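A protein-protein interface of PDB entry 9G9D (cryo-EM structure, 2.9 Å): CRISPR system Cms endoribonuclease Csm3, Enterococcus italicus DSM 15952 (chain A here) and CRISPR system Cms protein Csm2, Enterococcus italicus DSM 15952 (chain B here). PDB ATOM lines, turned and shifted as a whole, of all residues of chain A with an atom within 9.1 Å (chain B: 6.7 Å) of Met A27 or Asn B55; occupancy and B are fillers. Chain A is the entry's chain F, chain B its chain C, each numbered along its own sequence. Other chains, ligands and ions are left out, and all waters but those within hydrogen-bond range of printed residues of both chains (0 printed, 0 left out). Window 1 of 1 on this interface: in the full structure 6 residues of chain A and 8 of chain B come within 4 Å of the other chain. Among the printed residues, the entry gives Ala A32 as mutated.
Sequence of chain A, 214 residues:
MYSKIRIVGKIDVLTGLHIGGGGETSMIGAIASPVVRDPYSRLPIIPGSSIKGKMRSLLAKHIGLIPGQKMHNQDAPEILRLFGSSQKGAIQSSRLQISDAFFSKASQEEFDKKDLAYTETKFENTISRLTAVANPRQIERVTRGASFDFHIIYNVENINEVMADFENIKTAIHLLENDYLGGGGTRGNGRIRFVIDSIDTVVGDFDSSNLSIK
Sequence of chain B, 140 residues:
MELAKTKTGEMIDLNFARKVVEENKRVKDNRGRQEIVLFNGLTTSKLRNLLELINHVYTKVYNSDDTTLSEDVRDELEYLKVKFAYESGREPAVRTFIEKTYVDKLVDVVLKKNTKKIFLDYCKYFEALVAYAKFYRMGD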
ATOM      1  N   GLU A  24      -6.652  11.664  15.949  1.00  0.00           N
ATOM      2  CA  GLU A  24      -7.106  12.401  17.123  1.00  0.00           C
ATOM      3  C   GLU A  24      -7.228  13.883  16.792  1.00  0.00           C
ATOM      4  O   GLU A  24      -6.310  14.474  16.213  1.00  0.00           O
ATOM      5  CB  GLU A  24      -6.146  12.192  18.294  1.00  0.00           C
ATOM      6  CG  GLU A  24      -5.924  10.735  18.665  1.00  0.00           C
ATOM      7  CD  GLU A  24      -7.168  10.080  19.231  1.00  0.00           C
ATOM      8  OE1 GLU A  24      -8.040  10.803  19.756  1.00  0.00           O
ATOM      9  OE2 GLU A  24      -7.275   8.838  19.152  1.00  0.00           O
ATOM     10  N   THR A  25      -8.358  14.478  17.167  1.00  0.00           N
ATOM     11  CA  THR A  25      -8.575  15.915  17.065  1.00  0.00           C
ATOM     12  C   THR A  25      -8.536  16.518  18.463  1.00  0.00           C
ATOM     13  O   THR A  25      -9.175  15.998  19.383  1.00  0.00           O
ATOM     14  CB  THR A  25      -9.916  16.224  16.394  1.00  0.00           C
ATOM     15  OG1 THR A  25      -9.916  15.711  15.056  1.00  0.00           O
ATOM     16  CG2 THR A  25     -10.164  17.725  16.355  1.00  0.00           C
ATOM     17  N   SER A  26      -7.790  17.609  18.619  1.00  0.00           N
ATOM     18  CA  SER A  26      -7.590  18.221  19.924  1.00  0.00           C
ATOM     19  C   SER A  26      -7.856  19.716  19.830  1.00  0.00           C
ATOM     20  O   SER A  26      -7.916  20.293  18.742  1.00  0.00           O
ATOM     21  CB  SER A  26      -6.176  17.956  20.455  1.00  0.00           C
ATOM     22  OG  SER A  26      -5.199  18.427  19.545  1.00  0.00           O
ATOM     23  N   MET A  27      -8.013  20.341  20.994  1.00  0.00           N
ATOM     24  CA  MET A  27      -8.335  21.757  21.057  1.00  0.00           C
ATOM     25  C   MET A  27      -7.144  22.602  20.612  1.00  0.00           C
ATOM     26  O   MET A  27      -5.993  22.161  20.626  1.00  0.00           O
ATOM     27  CB  MET A  27      -8.772  22.139  22.474  1.00  0.00           C
ATOM     28  CG  MET A  27      -7.792  23.008  23.238  1.00  0.00           C
ATOM     29  SD  MET A  27      -8.388  23.459  24.879  1.00  0.00           S
ATOM     30  CE  MET A  27      -9.862  24.380  24.463  1.00  0.00           C
ATOM     31  N   ILE A  28      -7.442  23.830  20.188  1.00  0.00           N
ATOM     32  CA  ILE A  28      -6.420  24.770  19.739  1.00  0.00           C
ATOM     33  C   ILE A  28      -5.420  25.010  20.860  1.00  0.00           C
ATOM     34  O   ILE A  28      -5.793  25.433  21.960  1.00  0.00           O
ATOM     35  CB  ILE A  28      -7.051  26.094  19.276  1.00  0.00           C
ATOM     36  CG1 ILE A  28      -8.039  25.843  18.138  1.00  0.00           C
ATOM     37  CG2 ILE A  28      -5.972  27.074  18.853  1.00  0.00           C
ATOM     38  CD1 ILE A  28      -8.731  27.092  17.644  1.00  0.00           C
ATOM     39  N   GLY A  29      -4.143  24.745  20.590  1.00  0.00           N
ATOM     40  CA  GLY A  29      -3.101  24.901  21.582  1.00  0.00           C
ATOM     41  C   GLY A  29      -2.878  23.701  22.477  1.00  0.00           C
ATOM     42  O   GLY A  29      -1.963  23.734  23.309  1.00  0.00           O
ATOM     43  N   ALA A  30      -3.681  22.651  22.342  1.00  0.00           N
ATOM     44  CA  ALA A  30      -3.565  21.459  23.166  1.00  0.00           C
ATOM     45  C   ALA A  30      -2.588  20.476  22.523  1.00  0.00           C
ATOM     46  O   ALA A  30      -1.805  20.830  21.638  1.00  0.00           O
ATOM     47  CB  ALA A  30      -4.938  20.831  23.389  1.00  0.00           C
ATOM     48  N   ILE A  31      -2.618  19.226  22.990  1.00  0.00           N
ATOM     49  CA  ILE A  31      -1.676  18.210  22.531  1.00  0.00           C
ATOM     50  C   ILE A  31      -1.814  18.038  21.026  1.00  0.00           C
ATOM     51  O   ILE A  31      -2.924  17.905  20.498  1.00  0.00           O
ATOM     52  CB  ILE A  31      -1.911  16.889  23.269  1.00  0.00           C
ATOM     53  CG1 ILE A  31      -1.906  17.122  24.781  1.00  0.00           C
ATOM     54  CG2 ILE A  31      -0.858  15.863  22.880  1.00  0.00           C
ATOM     55  CD1 ILE A  31      -2.248  15.893  25.583  1.00  0.00           C
ATOM     56  N   ALA A  32      -0.679  18.038  20.326  1.00  0.00           N
ATOM     57  CA  ALA A  32      -0.714  17.956  18.871  1.00  0.00           C
ATOM     58  C   ALA A  32      -0.513  16.529  18.376  1.00  0.00           C
ATOM     59  O   ALA A  32      -1.225  16.080  17.471  1.00  0.00           O
ATOM     60  CB  ALA A  32       0.342  18.886  18.268  1.00  0.00           C
ATOM     61  N   THR A 121       3.258  15.432  28.477  1.00  0.00           N
ATOM     62  CA  THR A 121       3.188  16.303  27.308  1.00  0.00           C
ATOM     63  C   THR A 121       4.483  17.101  27.249  1.00  0.00           C
ATOM     64  O   THR A 121       4.664  18.069  27.991  1.00  0.00           O
ATOM     65  CB  THR A 121       1.966  17.213  27.373  1.00  0.00           C
ATOM     66  OG1 THR A 121       0.778  16.414  27.429  1.00  0.00           O
ATOM     67  CG2 THR A 121       1.906  18.104  26.148  1.00  0.00           C
ATOM     68  N   PHE A 123       6.890  19.770  25.705  1.00  0.00           N
ATOM     69  CA  PHE A 123       6.738  21.019  24.976  1.00  0.00           C
ATOM     70  C   PHE A 123       8.033  21.325  24.241  1.00  0.00           C
ATOM     71  O   PHE A 123       9.090  21.443  24.865  1.00  0.00           O
ATOM     72  CB  PHE A 123       6.373  22.163  25.921  1.00  0.00           C
ATOM     73  CG  PHE A 123       4.955  22.115  26.403  1.00  0.00           C
ATOM     74  CD1 PHE A 123       4.560  21.193  27.355  1.00  0.00           C
ATOM     75  CD2 PHE A 123       4.016  22.994  25.902  1.00  0.00           C
ATOM     76  CE1 PHE A 123       3.255  21.148  27.796  1.00  0.00           C
ATOM     77  CE2 PHE A 123       2.709  22.956  26.342  1.00  0.00           C
ATOM     78  CZ  PHE A 123       2.328  22.032  27.289  1.00  0.00           C
ATOM     79  N   GLN A 138       3.514  20.185  20.903  1.00  0.00           N
ATOM     80  CA  GLN A 138       3.349  19.400  22.118  1.00  0.00           C
ATOM     81  C   GLN A 138       3.248  17.930  21.742  1.00  0.00           C
ATOM     82  O   GLN A 138       2.307  17.524  21.051  1.00  0.00           O
ATOM     83  CB  GLN A 138       2.106  19.837  22.894  1.00  0.00           C
ATOM     84  CG  GLN A 138       2.069  21.317  23.226  1.00  0.00           C
ATOM     85  CD  GLN A 138       0.779  21.724  23.907  1.00  0.00           C
ATOM     86  OE1 GLN A 138       0.046  20.883  24.425  1.00  0.00           O
ATOM     87  NE2 GLN A 138       0.493  23.020  23.906  1.00  0.00           N
ATOM     88  N   ARG B  48      -4.421  34.197  24.505  1.00  0.00           N
ATOM     89  CA  ARG B  48      -3.672  32.947  24.544  1.00  0.00           C
ATOM     90  C   ARG B  48      -3.384  32.508  25.971  1.00  0.00           C
ATOM     91  O   ARG B  48      -3.320  31.309  26.242  1.00  0.00           O
ATOM     92  CB  ARG B  48      -2.370  33.075  23.755  1.00  0.00           C
ATOM     93  CG  ARG B  48      -2.564  33.135  22.248  1.00  0.00           C
ATOM     94  CD  ARG B  48      -3.707  32.235  21.795  1.00  0.00           C
ATOM     95  NE  ARG B  48      -3.435  30.820  22.022  1.00  0.00           N
ATOM     96  CZ  ARG B  48      -3.090  29.962  21.072  1.00  0.00           C
ATOM     97  NH1 ARG B  48      -2.975  30.339  19.810  1.00  0.00           N
ATOM     98  NH2 ARG B  48      -2.856  28.694  21.397  1.00  0.00           N
ATOM     99  N   LEU B  50      -5.474  33.093  28.559  1.00  0.00           N
ATOM    100  CA  LEU B  50      -6.747  32.513  28.973  1.00  0.00           C
ATOM    101  C   LEU B  50      -6.953  31.146  28.327  1.00  0.00           C
ATOM    102  O   LEU B  50      -7.426  30.202  28.975  1.00  0.00           O
ATOM    103  CB  LEU B  50      -7.894  33.460  28.622  1.00  0.00           C
ATOM    104  CG  LEU B  50      -7.816  34.876  29.197  1.00  0.00           C
ATOM    105  CD1 LEU B  50      -8.991  35.705  28.717  1.00  0.00           C
ATOM    106  CD2 LEU B  50      -7.775  34.843  30.713  1.00  0.00           C
ATOM    107  N   LEU B  51      -6.572  31.017  27.057  1.00  0.00           N
ATOM    108  CA  LEU B  51      -6.675  29.739  26.373  1.00  0.00           C
ATOM    109  C   LEU B  51      -5.713  28.711  26.953  1.00  0.00           C
ATOM    110  O   LEU B  51      -5.990  27.518  26.892  1.00  0.00           O
ATOM    111  CB  LEU B  51      -6.421  29.924  24.880  1.00  0.00           C
ATOM    112  CG  LEU B  51      -6.647  28.699  23.997  1.00  0.00           C
ATOM    113  CD1 LEU B  51      -8.087  28.220  24.096  1.00  0.00           C
ATOM    114  CD2 LEU B  51      -6.278  29.024  22.565  1.00  0.00           C
ATOM    115  N   GLU B  52      -4.580  29.145  27.505  1.00  0.00           N
ATOM    116  CA  GLU B  52      -3.671  28.207  28.158  1.00  0.00           C
ATOM    117  C   GLU B  52      -4.283  27.668  29.444  1.00  0.00           C
ATOM    118  O   GLU B  52      -4.171  26.472  29.749  1.00  0.00           O
ATOM    119  CB  GLU B  52      -2.327  28.884  28.436  1.00  0.00           C
ATOM    120  CG  GLU B  52      -1.173  27.918  28.683  1.00  0.00           C
ATOM    121  CD  GLU B  52      -1.168  27.337  30.088  1.00  0.00           C
ATOM    122  OE1 GLU B  52      -1.140  28.124  31.057  1.00  0.00           O
ATOM    123  OE2 GLU B  52      -1.196  26.096  30.224  1.00  0.00           O
ATOM    124  N   LEU B  53      -4.965  28.544  30.183  1.00  0.00           N
ATOM    125  CA  LEU B  53      -5.691  28.065  31.383  1.00  0.00           C
ATOM    126  C   LEU B  53      -6.698  27.018  30.902  1.00  0.00           C
ATOM    127  O   LEU B  53      -6.703  25.897  31.448  1.00  0.00           O
ATOM    128  CB  LEU B  53      -6.403  29.234  32.060  1.00  0.00           C
ATOM    129  CG  LEU B  53      -5.530  30.440  32.417  1.00  0.00           C
ATOM    130  CD1 LEU B  53      -6.386  31.585  32.929  1.00  0.00           C
ATOM    131  CD2 LEU B  53      -4.472  30.059  33.437  1.00  0.00           C
ATOM    132  N   ILE B  54      -7.497  27.375  29.894  1.00  0.00           N
ATOM    133  CA  ILE B  54      -8.502  26.454  29.373  1.00  0.00           C
ATOM    134  C   ILE B  54      -7.854  25.165  28.891  1.00  0.00           C
ATOM    135  O   ILE B  54      -8.422  24.084  29.055  1.00  0.00           O
ATOM    136  CB  ILE B  54      -9.315  27.130  28.253  1.00  0.00           C
ATOM    137  CG1 ILE B  54     -10.004  28.386  28.779  1.00  0.00           C
ATOM    138  CG2 ILE B  54     -10.356  26.175  27.699  1.00  0.00           C
ATOM    139  CD1 ILE B  54     -11.066  28.102  29.804  1.00  0.00           C
ATOM    140  N   ASN B  55      -6.667  25.254  28.288  1.00  0.00           N
ATOM    141  CA  ASN B  55      -5.971  24.070  27.799  1.00  0.00           C
ATOM    142  C   ASN B  55      -5.626  23.132  28.940  1.00  0.00           C
ATOM    143  O   ASN B  55      -5.799  21.915  28.831  1.00  0.00           O
ATOM    144  CB  ASN B  55      -4.698  24.474  27.054  1.00  0.00           C
ATOM    145  CG  ASN B  55      -4.962  24.900  25.629  1.00  0.00           C
ATOM    146  OD1 ASN B  55      -5.264  24.074  24.770  1.00  0.00           O
ATOM    147  ND2 ASN B  55      -4.829  26.191  25.363  1.00  0.00           N
ATOM    148  N   HIS B  56      -5.107  23.680  30.038  1.00  0.00           N
ATOM    149  CA  HIS B  56      -4.757  22.832  31.172  1.00  0.00           C
ATOM    150  C   HIS B  56      -5.995  22.142  31.733  1.00  0.00           C
ATOM    151  O   HIS B  56      -5.997  20.922  31.962  1.00  0.00           O
ATOM    152  CB  HIS B  56      -4.057  23.651  32.255  1.00  0.00           C
ATOM    153  CG  HIS B  56      -3.605  22.835  33.426  1.00  0.00           C
ATOM    154  ND1 HIS B  56      -3.480  23.358  34.695  1.00  0.00           N
ATOM    155  CD2 HIS B  56      -3.250  21.531  33.520  1.00  0.00           C
ATOM    156  CE1 HIS B  56      -3.069  22.412  35.521  1.00  0.00           C
ATOM    157  NE2 HIS B  56      -2.921  21.295  34.833  1.00  0.00           N
ATOM    158  N   VAL B  57      -7.073  22.898  31.928  1.00  0.00           N
ATOM    159  CA  VAL B  57      -8.306  22.288  32.514  1.00  0.00           C
ATOM    160  C   VAL B  57      -8.861  21.264  31.508  1.00  0.00           C
ATOM    161  O   VAL B  57      -9.365  20.212  31.958  1.00  0.00           O
ATOM    162  CB  VAL B  57      -9.369  23.335  32.903  1.00  0.00           C
ATOM    163  CG1 VAL B  57     -10.468  22.727  33.765  1.00  0.00           C
ATOM    164  CG2 VAL B  57      -8.747  24.529  33.617  1.00  0.00           C
ATOM    165  N   TYR B  58      -8.753  21.543  30.204  1.00  0.00           N
ATOM    166  CA  TYR B  58      -9.295  20.649  29.188  1.00  0.00           C
ATOM    167  C   TYR B  58      -8.505  19.354  29.115  1.00  0.00           C
ATOM    168  O   TYR B  58      -9.079  18.279  28.946  1.00  0.00           O
ATOM    169  CB  TYR B  58      -9.300  21.350  27.830  1.00  0.00           C
ATOM    170  CG  TYR B  58      -9.331  20.402  26.655  1.00  0.00           C
ATOM    171  CD1 TYR B  58     -10.500  19.748  26.299  1.00  0.00           C
ATOM    172  CD2 TYR B  58      -8.190  20.164  25.900  1.00  0.00           C
ATOM    173  CE1 TYR B  58     -10.534  18.882  25.226  1.00  0.00           C
ATOM    174  CE2 TYR B  58      -8.214  19.299  24.824  1.00  0.00           C
ATOM    175  CZ  TYR B  58      -9.390  18.661  24.492  1.00  0.00           C
ATOM    176  OH  TYR B  58      -9.425  17.799  23.422  1.00  0.00           O
ATOM    177  N   THR B  59      -7.179  19.441  29.209  1.00  0.00           N
ATOM    178  CA  THR B  59      -6.368  18.231  29.263  1.00  0.00           C
ATOM    179  C   THR B  59      -6.720  17.405  30.491  1.00  0.00           C
ATOM    180  O   THR B  59      -6.887  16.179  30.404  1.00  0.00           O
ATOM    181  CB  THR B  59      -4.882  18.596  29.263  1.00  0.00           C
ATOM    182  OG1 THR B  59      -4.580  19.369  28.095  1.00  0.00           O
ATOM    183  CG2 THR B  59      -4.018  17.344  29.270  1.00  0.00           C
ATOM    184  N   LYS B  60      -6.870  18.070  31.642  1.00  0.00           N
ATOM    185  CA  LYS B  60      -7.220  17.360  32.867  1.00  0.00           C
ATOM    186  C   LYS B  60      -8.544  16.618  32.716  1.00  0.00           C
ATOM    187  O   LYS B  60      -8.674  15.466  33.145  1.00  0.00           O
ATOM    188  CB  LYS B  60      -7.282  18.339  34.040  1.00  0.00           C
ATOM    189  CG  LYS B  60      -7.692  17.706  35.360  1.00  0.00           C
ATOM    190  CD  LYS B  60      -6.729  16.603  35.769  1.00  0.00           C
ATOM    191  CE  LYS B  60      -7.155  15.952  37.076  1.00  0.00           C
ATOM    192  NZ  LYS B  60      -6.218  14.875  37.497  1.00  0.00           N
ATOM    193  N   TYR B  62     -10.124  15.817  29.814  1.00  0.00           N
ATOM    194  CA  TYR B  62     -10.105  14.879  28.696  1.00  0.00           C
ATOM    195  C   TYR B  62      -9.438  13.572  29.094  1.00  0.00           C
ATOM    196  O   TYR B  62      -9.887  12.491  28.694  1.00  0.00           O
ATOM    197  CB  TYR B  62      -9.388  15.509  27.501  1.00  0.00           C
ATOM    198  CG  TYR B  62      -9.701  14.859  26.172  1.00  0.00           C
ATOM    199  CD1 TYR B  62     -10.764  13.977  26.041  1.00  0.00           C
ATOM    200  CD2 TYR B  62      -8.927  15.125  25.050  1.00  0.00           C
ATOM    201  CE1 TYR B  62     -11.052  13.380  24.828  1.00  0.00           C
ATOM    202  CE2 TYR B  62      -9.207  14.533  23.832  1.00  0.00           C
ATOM    203  CZ  TYR B  62     -10.271  13.661  23.728  1.00  0.00           C
ATOM    204  OH  TYR B  62     -10.554  13.069  22.519  1.00  0.00           O
ATOM    205  N   TYR B 122     -17.974  24.158  26.031  1.00  0.00           N
ATOM    206  CA  TYR B 122     -17.390  25.463  26.443  1.00  0.00           C
ATOM    207  C   TYR B 122     -15.972  25.557  25.891  1.00  0.00           C
ATOM    208  O   TYR B 122     -15.573  26.635  25.403  1.00  0.00           O
ATOM    209  CB  TYR B 122     -17.428  25.624  27.966  1.00  0.00           C
ATOM    210  CG  TYR B 122     -16.555  26.753  28.496  1.00  0.00           C
ATOM    211  CD1 TYR B 122     -16.928  28.080  28.335  1.00  0.00           C
ATOM    212  CD2 TYR B 122     -15.373  26.492  29.176  1.00  0.00           C
ATOM    213  CE1 TYR B 122     -16.146  29.115  28.816  1.00  0.00           C
ATOM    214  CE2 TYR B 122     -14.583  27.518  29.666  1.00  0.00           C
ATOM    215  CZ  TYR B 122     -14.970  28.832  29.486  1.00  0.00           C
ATOM    216  OH  TYR B 122     -14.197  29.850  29.964  1.00  0.00           O
ATOM    217  N   CYS B 123     -15.222  24.456  25.968  1.00  0.00           N
ATOM    218  CA  CYS B 123     -13.852  24.449  25.393  1.00  0.00           C
ATOM    219  C   CYS B 123     -13.950  24.865  23.920  1.00  0.00           C
ATOM    220  O   CYS B 123     -13.168  25.742  23.503  1.00  0.00           O
ATOM    221  CB  CYS B 123     -13.218  23.072  25.536  1.00  0.00           C
ATOM    222  SG  CYS B 123     -13.080  22.521  27.255  1.00  0.00           S
ATOM    223  N   LYS B 124     -14.898  24.282  23.180  1.00  0.00           N
ATOM    224  CA  LYS B 124     -15.086  24.620  21.774  1.00  0.00           C
ATOM    225  C   LYS B 124     -15.532  26.065  21.602  1.00  0.00           C
ATOM    226  O   LYS B 124     -15.163  26.712  20.619  1.00  0.00           O
ATOM    227  CB  LYS B 124     -16.092  23.669  21.127  1.00  0.00           C
ATOM    228  CG  LYS B 124     -15.614  22.230  21.065  1.00  0.00           C
ATOM    229  CD  LYS B 124     -16.130  21.520  19.827  1.00  0.00           C
ATOM    230  CE  LYS B 124     -15.585  20.104  19.747  1.00  0.00           C
ATOM    231  NZ  LYS B 124     -14.103  20.074  19.891  1.00  0.00           N
ATOM    232  N   PHE B 126     -14.612  28.560  23.576  1.00  0.00           N
ATOM    233  CA  PHE B 126     -13.368  29.350  23.774  1.00  0.00           C
ATOM    234  C   PHE B 126     -12.521  29.249  22.512  1.00  0.00           C
ATOM    235  O   PHE B 126     -11.966  30.275  22.070  1.00  0.00           O
ATOM    236  CB  PHE B 126     -12.608  28.851  25.004  1.00  0.00           C
ATOM    237  CG  PHE B 126     -11.982  29.969  25.827  1.00  0.00           C
ATOM    238  CD1 PHE B 126     -10.728  30.476  25.506  1.00  0.00           C
ATOM    239  CD2 PHE B 126     -12.650  30.507  26.919  1.00  0.00           C
ATOM    240  CE1 PHE B 126     -10.164  31.495  26.257  1.00  0.00           C
ATOM    241  CE2 PHE B 126     -12.079  31.524  27.668  1.00  0.00           C
ATOM    242  CZ  PHE B 126     -10.841  32.015  27.334  1.00  0.00           C
ATOM    243  N   GLU B 127     -12.417  28.045  21.944  1.00  0.00           N
ATOM    244  CA  GLU B 127     -11.669  27.863  20.706  1.00  0.00           C
ATOM    245  C   GLU B 127     -12.239  28.733  19.597  1.00  0.00           C
ATOM    246  O   GLU B 127     -11.495  29.329  18.817  1.00  0.00           O
ATOM    247  CB  GLU B 127     -11.690  26.396  20.279  1.00  0.00           C
ATOM    248  CG  GLU B 127     -10.961  25.451  21.200  1.00  0.00           C
ATOM    249  CD  GLU B 127     -10.927  24.040  20.652  1.00  0.00           C
ATOM    250  OE1 GLU B 127     -10.299  23.833  19.592  1.00  0.00           O
ATOM    251  OE2 GLU B 127     -11.537  23.142  21.269  1.00  0.00           O
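The side-chain amide nitrogen (NE2) of Gln A138 lies within hydrogen-bond range of the backbone carbonyl oxygen (O) of Gly A29 (2.6 Å). The side-chain hydroxyl (OG) of Ser A26 is in hydrogen-bond range of the backbone carbonyl oxygen (O) of Ile A31, at 2.5 Å. O of Ala A30 lies close to OE1 of Gln A138 (3.3 Å). O of Asn B55 sits at hydrogen-bond distance from OG1 of Thr B59 (2.9 Å).
OD1 of Asn B55 lies close to O of Ile A28, 3.2 Å away. OD1 of Asn B55 lies within hydrogen-bond range of N of Ala A30, at 3.2 Å. N of Ile A28 sits at hydrogen-bond distance from OE1 of Glu B127, at 2.9 Å. The side-chain amide oxygen (OD1) of Asn B55 sits close to the side-chain sulfur (SD) of Met A27, at 3.2 Å.
Of the 12 printed residues of chain A, 5 touch a printed residue of chain B. Along chain A the printed residues that touch a printed residue of chain B span positions 26 to 30. Of the 18 printed residues of chain B, 7 touch a printed residue of chain A. Hydrophobic or aromatic side chains of chain B within 4 Å of the printed part of chain A: Leu B51, Ile B54 and Tyr B58. Among the printed residues, no Asp or Glu carboxylate lies within 4 Å of a Lys or Arg side-chain nitrogen of the other chain.
OH of Tyr B58 touches CA of Ser A26, 3.97 Å away. Ile B54 touches Met A27 (CG2 to CE, 3.7 Å). Met A27 touches Tyr B58 (SD to CD2, 3.5 Å). CE of Met A27 touches O of Cys B123, 3.7 Å away. Met A27 touches Glu B127. Leu B51 touches Ile A28. NH2 of Arg B48 touches CA of Gly A29, 3.8 Å away. OD1 of Asn B55 touches C of Gly A29, 3.3 Å away. Tyr B58 touches Ala A30.
Of the printed residues of chain B, Ser A26 touches Tyr B58 (3.97 Å). Met A27 touches five residues of chain B. Of the printed residues of chain B, Ala A30 touches Asn B55 (3.2 Å) and Tyr B58 (3.9 Å). Of the printed residues of chain A, Tyr B58 touches Ser A26, Met A27 and Ala A30. Lys B60 touches none of the printed residues of chain A.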
